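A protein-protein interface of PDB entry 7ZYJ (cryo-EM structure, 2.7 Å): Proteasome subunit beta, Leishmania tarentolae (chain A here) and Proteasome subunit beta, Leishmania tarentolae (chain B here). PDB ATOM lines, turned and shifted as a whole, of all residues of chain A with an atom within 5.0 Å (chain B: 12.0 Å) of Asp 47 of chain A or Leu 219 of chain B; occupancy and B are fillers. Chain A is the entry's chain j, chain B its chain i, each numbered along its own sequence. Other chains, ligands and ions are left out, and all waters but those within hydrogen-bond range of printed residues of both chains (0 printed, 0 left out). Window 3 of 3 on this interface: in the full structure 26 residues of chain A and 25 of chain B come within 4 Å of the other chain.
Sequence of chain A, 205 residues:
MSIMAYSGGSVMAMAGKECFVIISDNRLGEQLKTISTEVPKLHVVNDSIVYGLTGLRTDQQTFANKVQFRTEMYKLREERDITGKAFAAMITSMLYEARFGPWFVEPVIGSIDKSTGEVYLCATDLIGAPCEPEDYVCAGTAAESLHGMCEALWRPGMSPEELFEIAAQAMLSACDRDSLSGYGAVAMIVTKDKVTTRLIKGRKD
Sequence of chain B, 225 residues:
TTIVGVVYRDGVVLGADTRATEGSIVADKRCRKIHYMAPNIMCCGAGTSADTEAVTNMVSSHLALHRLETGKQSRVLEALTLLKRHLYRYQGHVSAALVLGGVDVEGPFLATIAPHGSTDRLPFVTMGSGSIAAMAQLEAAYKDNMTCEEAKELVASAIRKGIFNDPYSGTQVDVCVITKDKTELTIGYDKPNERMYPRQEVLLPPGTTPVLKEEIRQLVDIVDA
Of the printed residues of chain B, Asp 47 of chain A touches Leu 219 (3.7 Å).
No residue of chain B comes within 4 Å of Asn 46 of chain A.
No residue of chain B comes within 4 Å of Ser 48 of chain A.
No residue of chain B comes within 4 Å of Ile 49 of chain A.
Asp 193 of chain A touches just these residues of chain B: Gln 218 and Leu 219.
Printed residues of chain A within 4 Å of Ile 216 of chain B: Lys 194 and Val 195.
Of the printed residues of chain A, Arg 217 of chain B touches Lys 194 (3.5 Å) and Val 195 (2.6 Å).
Printed residues of chain B within 4 Å of Lys 194 of chain A: Ile 216 (3.9 Å), Arg 217 (3.5 Å) and Gln 218 (3.4 Å).
Val 45 of chain A touches none of the printed residues of chain B.
The nearest residue of chain A that does not touch Leu 219 of chain B is Lys 194 of chain A (4.2 Å).
The backbone carbonyl oxygen (O) of Asp 193 of chain A lies within hydrogen-bond range of the backbone NH (N) of Leu 219 of chain B, at 2.9 Å.
The backbone carbonyl oxygen (O) of Val 195 of chain A sits at hydrogen-bond distance from the backbone NH (N) of Arg 217 of chain B, 2.6 Å away.
Of the 10 printed residues of chain A, 5 touch a printed residue of chain B.
Hydrophobic or aromatic side chains of chain A that line the printed part of chain B: Val 195.
Hydrophobic or aromatic side chains of chain B within 4 Å of the printed part of chain A: Ile 216 and Leu 219.
Leu 219 of chain B touches Asp 47 of chain A (CD1 to CB, 3.7 Å).
Lys 114 of chain A touches Leu 219 of chain B (NZ to CD1, 3.4 Å).
Asp 193 of chain A touches Gln 218 of chain B (O to C, 3.97 Å).
CG2 of Ile 216 of chain B touches CD of Lys 194 of chain A (3.9 Å).
CA of Lys 194 of chain A touches O of Arg 217 of chain B (3.5 Å).
CD of Lys 194 of chain A touches NE2 of Gln 218 of chain B, at 3.4 Å.
Val 195 of chain A touches Ile 216 of chain B.
CG2 of Val 195 of chain A touches CD1 of Leu 219 of chain B (3.6 Å).
The side-chain carboxylate (OD2) of Asp 193 of chain A is in salt-bridge range of the side-chain amino group (NZ) of Lys 194 of chain A (3.9 Å).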
ATOM      1  N   VAL A  45      -3.884 -15.569 -24.873  1.00  0.00           N
ATOM      2  CA  VAL A  45      -3.323 -16.866 -24.512  1.00  0.00           C
ATOM      3  C   VAL A  45      -1.809 -16.786 -24.365  1.00  0.00           C
ATOM      4  O   VAL A  45      -1.247 -17.285 -23.389  1.00  0.00           O
ATOM      5  CB  VAL A  45      -3.735 -17.922 -25.556  1.00  0.00           C
ATOM      6  CG1 VAL A  45      -3.010 -19.232 -25.304  1.00  0.00           C
ATOM      7  CG2 VAL A  45      -5.234 -18.122 -25.525  1.00  0.00           C
ATOM      8  N   ASN A  46      -1.141 -16.154 -25.319  1.00  0.00           N
ATOM      9  CA  ASN A  46       0.306 -15.969 -25.297  1.00  0.00           C
ATOM     10  C   ASN A  46       0.630 -14.807 -26.230  1.00  0.00           C
ATOM     11  O   ASN A  46      -0.267 -14.079 -26.672  1.00  0.00           O
ATOM     12  CB  ASN A  46       1.042 -17.253 -25.688  1.00  0.00           C
ATOM     13  CG  ASN A  46       0.617 -17.781 -27.042  1.00  0.00           C
ATOM     14  OD1 ASN A  46       0.925 -17.192 -28.077  1.00  0.00           O
ATOM     15  ND2 ASN A  46      -0.094 -18.901 -27.042  1.00  0.00           N
ATOM     16  N   ASP A  47       1.915 -14.634 -26.533  1.00  0.00           N
ATOM     17  CA  ASP A  47       2.351 -13.529 -27.377  1.00  0.00           C
ATOM     18  C   ASP A  47       1.842 -13.636 -28.808  1.00  0.00           C
ATOM     19  O   ASP A  47       1.930 -12.653 -29.551  1.00  0.00           O
ATOM     20  CB  ASP A  47       3.878 -13.448 -27.380  1.00  0.00           C
ATOM     21  CG  ASP A  47       4.440 -13.016 -26.040  1.00  0.00           C
ATOM     22  OD1 ASP A  47       3.744 -12.275 -25.314  1.00  0.00           O
ATOM     23  OD2 ASP A  47       5.576 -13.416 -25.712  1.00  0.00           O
ATOM     24  N   SER A  48       1.318 -14.791 -29.214  1.00  0.00           N
ATOM     25  CA  SER A  48       0.898 -14.998 -30.593  1.00  0.00           C
ATOM     26  C   SER A  48      -0.600 -15.175 -30.784  1.00  0.00           C
ATOM     27  O   SER A  48      -1.092 -14.885 -31.880  1.00  0.00           O
ATOM     28  CB  SER A  48       1.608 -16.225 -31.187  1.00  0.00           C
ATOM     29  OG  SER A  48       3.012 -16.043 -31.201  1.00  0.00           O
ATOM     30  N   ILE A  49      -1.343 -15.623 -29.775  1.00  0.00           N
ATOM     31  CA  ILE A  49      -2.748 -15.980 -29.928  1.00  0.00           C
ATOM     32  C   ILE A  49      -3.592 -15.054 -29.066  1.00  0.00           C
ATOM     33  O   ILE A  49      -3.314 -14.886 -27.872  1.00  0.00           O
ATOM     34  CB  ILE A  49      -3.005 -17.450 -29.546  1.00  0.00           C
ATOM     35  CG1 ILE A  49      -2.039 -18.374 -30.287  1.00  0.00           C
ATOM     36  CG2 ILE A  49      -4.444 -17.832 -29.841  1.00  0.00           C
ATOM     37  CD1 ILE A  49      -2.033 -19.783 -29.754  1.00  0.00           C
ATOM     38  N   LYS A 114       5.443 -16.130 -35.028  1.00  0.00           N
ATOM     39  CA  LYS A 114       6.438 -15.110 -34.713  1.00  0.00           C
ATOM     40  C   LYS A 114       7.661 -15.212 -35.615  1.00  0.00           C
ATOM     41  O   LYS A 114       8.346 -14.210 -35.841  1.00  0.00           O
ATOM     42  CB  LYS A 114       6.848 -15.213 -33.244  1.00  0.00           C
ATOM     43  CG  LYS A 114       5.782 -14.728 -32.276  1.00  0.00           C
ATOM     44  CD  LYS A 114       5.131 -13.445 -32.767  1.00  0.00           C
ATOM     45  CE  LYS A 114       4.708 -12.561 -31.610  1.00  0.00           C
ATOM     46  NZ  LYS A 114       4.257 -11.219 -32.076  1.00  0.00           N
ATOM     47  N   VAL A 190      -1.802  -7.260 -33.297  1.00  0.00           N
ATOM     48  CA  VAL A 190      -0.719  -8.199 -33.049  1.00  0.00           C
ATOM     49  C   VAL A 190       0.112  -8.299 -34.317  1.00  0.00           C
ATOM     50  O   VAL A 190      -0.397  -8.698 -35.373  1.00  0.00           O
ATOM     51  CB  VAL A 190      -1.244  -9.577 -32.620  1.00  0.00           C
ATOM     52  CG1 VAL A 190      -0.105 -10.447 -32.123  1.00  0.00           C
ATOM     53  CG2 VAL A 190      -2.303  -9.417 -31.541  1.00  0.00           C
ATOM     54  N   ASP A 193       6.511  -8.319 -34.246  1.00  0.00           N
ATOM     55  CA  ASP A 193       7.447  -7.779 -33.268  1.00  0.00           C
ATOM     56  C   ASP A 193       6.788  -7.248 -32.002  1.00  0.00           C
ATOM     57  O   ASP A 193       7.374  -7.373 -30.922  1.00  0.00           O
ATOM     58  CB  ASP A 193       8.281  -6.659 -33.901  1.00  0.00           C
ATOM     59  CG  ASP A 193       7.443  -5.458 -34.297  1.00  0.00           C
ATOM     60  OD1 ASP A 193       6.354  -5.655 -34.875  1.00  0.00           O
ATOM     61  OD2 ASP A 193       7.872  -4.316 -34.030  1.00  0.00           O
ATOM     62  N   LYS A 194       5.598  -6.658 -32.094  1.00  0.00           N
ATOM     63  CA  LYS A 194       4.991  -6.023 -30.934  1.00  0.00           C
ATOM     64  C   LYS A 194       3.494  -6.291 -30.918  1.00  0.00           C
ATOM     65  O   LYS A 194       2.901  -6.693 -31.923  1.00  0.00           O
ATOM     66  CB  LYS A 194       5.246  -4.512 -30.917  1.00  0.00           C
ATOM     67  CG  LYS A 194       4.604  -3.768 -32.075  1.00  0.00           C
ATOM     68  CD  LYS A 194       4.937  -2.287 -32.039  1.00  0.00           C
ATOM     69  CE  LYS A 194       4.269  -1.545 -33.184  1.00  0.00           C
ATOM     70  NZ  LYS A 194       4.827  -1.947 -34.505  1.00  0.00           N
ATOM     71  N   VAL A 195       2.891  -6.060 -29.754  1.00  0.00           N
ATOM     72  CA  VAL A 195       1.448  -6.150 -29.567  1.00  0.00           C
ATOM     73  C   VAL A 195       0.967  -4.841 -28.960  1.00  0.00           C
ATOM     74  O   VAL A 195       1.512  -4.382 -27.950  1.00  0.00           O
ATOM     75  CB  VAL A 195       1.056  -7.339 -28.670  1.00  0.00           C
ATOM     76  CG1 VAL A 195      -0.436  -7.331 -28.409  1.00  0.00           C
ATOM     77  CG2 VAL A 195       1.473  -8.646 -29.313  1.00  0.00           C
ATOM     78  N   GLU B 215      -1.819   1.162 -25.350  1.00  0.00           N
ATOM     79  CA  GLU B 215      -0.733   0.459 -24.670  1.00  0.00           C
ATOM     80  C   GLU B 215       0.006  -0.385 -25.697  1.00  0.00           C
ATOM     81  O   GLU B 215      -0.606  -1.212 -26.380  1.00  0.00           O
ATOM     82  CB  GLU B 215      -1.256  -0.411 -23.524  1.00  0.00           C
ATOM     83  CG  GLU B 215      -1.987   0.356 -22.435  1.00  0.00           C
ATOM     84  CD  GLU B 215      -1.812  -0.268 -21.063  1.00  0.00           C
ATOM     85  OE1 GLU B 215      -1.665  -1.506 -20.985  1.00  0.00           O
ATOM     86  OE2 GLU B 215      -1.822   0.481 -20.063  1.00  0.00           O
ATOM     87  N   ILE B 216       1.316  -0.179 -25.806  1.00  0.00           N
ATOM     88  CA  ILE B 216       2.161  -0.912 -26.741  1.00  0.00           C
ATOM     89  C   ILE B 216       3.084  -1.824 -25.947  1.00  0.00           C
ATOM     90  O   ILE B 216       3.731  -1.382 -24.988  1.00  0.00           O
ATOM     91  CB  ILE B 216       2.968   0.047 -27.632  1.00  0.00           C
ATOM     92  CG1 ILE B 216       2.031   1.007 -28.368  1.00  0.00           C
ATOM     93  CG2 ILE B 216       3.813  -0.733 -28.627  1.00  0.00           C
ATOM     94  CD1 ILE B 216       2.737   2.177 -29.013  1.00  0.00           C
ATOM     95  N   ARG B 217       3.150  -3.094 -26.342  1.00  0.00           N
ATOM     96  CA  ARG B 217       3.981  -4.087 -25.668  1.00  0.00           C
ATOM     97  C   ARG B 217       4.918  -4.716 -26.691  1.00  0.00           C
ATOM     98  O   ARG B 217       4.476  -5.483 -27.553  1.00  0.00           O
ATOM     99  CB  ARG B 217       3.125  -5.154 -24.986  1.00  0.00           C
ATOM    100  CG  ARG B 217       2.461  -4.687 -23.701  1.00  0.00           C
ATOM    101  CD  ARG B 217       3.452  -3.977 -22.794  1.00  0.00           C
ATOM    102  NE  ARG B 217       2.797  -3.358 -21.648  1.00  0.00           N
ATOM    103  CZ  ARG B 217       2.821  -3.849 -20.416  1.00  0.00           C
ATOM    104  NH1 ARG B 217       3.463  -4.970 -20.132  1.00  0.00           N
ATOM    105  NH2 ARG B 217       2.185  -3.199 -19.446  1.00  0.00           N
ATOM    106  N   GLN B 218       6.204  -4.393 -26.594  1.00  0.00           N
ATOM    107  CA  GLN B 218       7.204  -4.971 -27.478  1.00  0.00           C
ATOM    108  C   GLN B 218       7.514  -6.407 -27.072  1.00  0.00           C
ATOM    109  O   GLN B 218       7.512  -6.756 -25.888  1.00  0.00           O
ATOM    110  CB  GLN B 218       8.486  -4.139 -27.455  1.00  0.00           C
ATOM    111  CG  GLN B 218       8.292  -2.678 -27.825  1.00  0.00           C
ATOM    112  CD  GLN B 218       7.854  -2.493 -29.263  1.00  0.00           C
ATOM    113  OE1 GLN B 218       8.277  -3.231 -30.153  1.00  0.00           O
ATOM    114  NE2 GLN B 218       7.003  -1.502 -29.499  1.00  0.00           N
ATOM    115  N   LEU B 219       7.784  -7.239 -28.071  1.00  0.00           N
ATOM    116  CA  LEU B 219       8.132  -8.635 -27.828  1.00  0.00           C
ATOM    117  C   LEU B 219       9.508  -8.963 -28.398  1.00  0.00           C
ATOM    118  O   LEU B 219      10.511  -8.926 -27.685  1.00  0.00           O
ATOM    119  CB  LEU B 219       7.079  -9.566 -28.430  1.00  0.00           C
ATOM    120  CG  LEU B 219       5.614  -9.200 -28.184  1.00  0.00           C
ATOM    121  CD1 LEU B 219       4.706 -10.190 -28.880  1.00  0.00           C
ATOM    122  CD2 LEU B 219       5.311  -9.149 -26.695  1.00  0.00           C
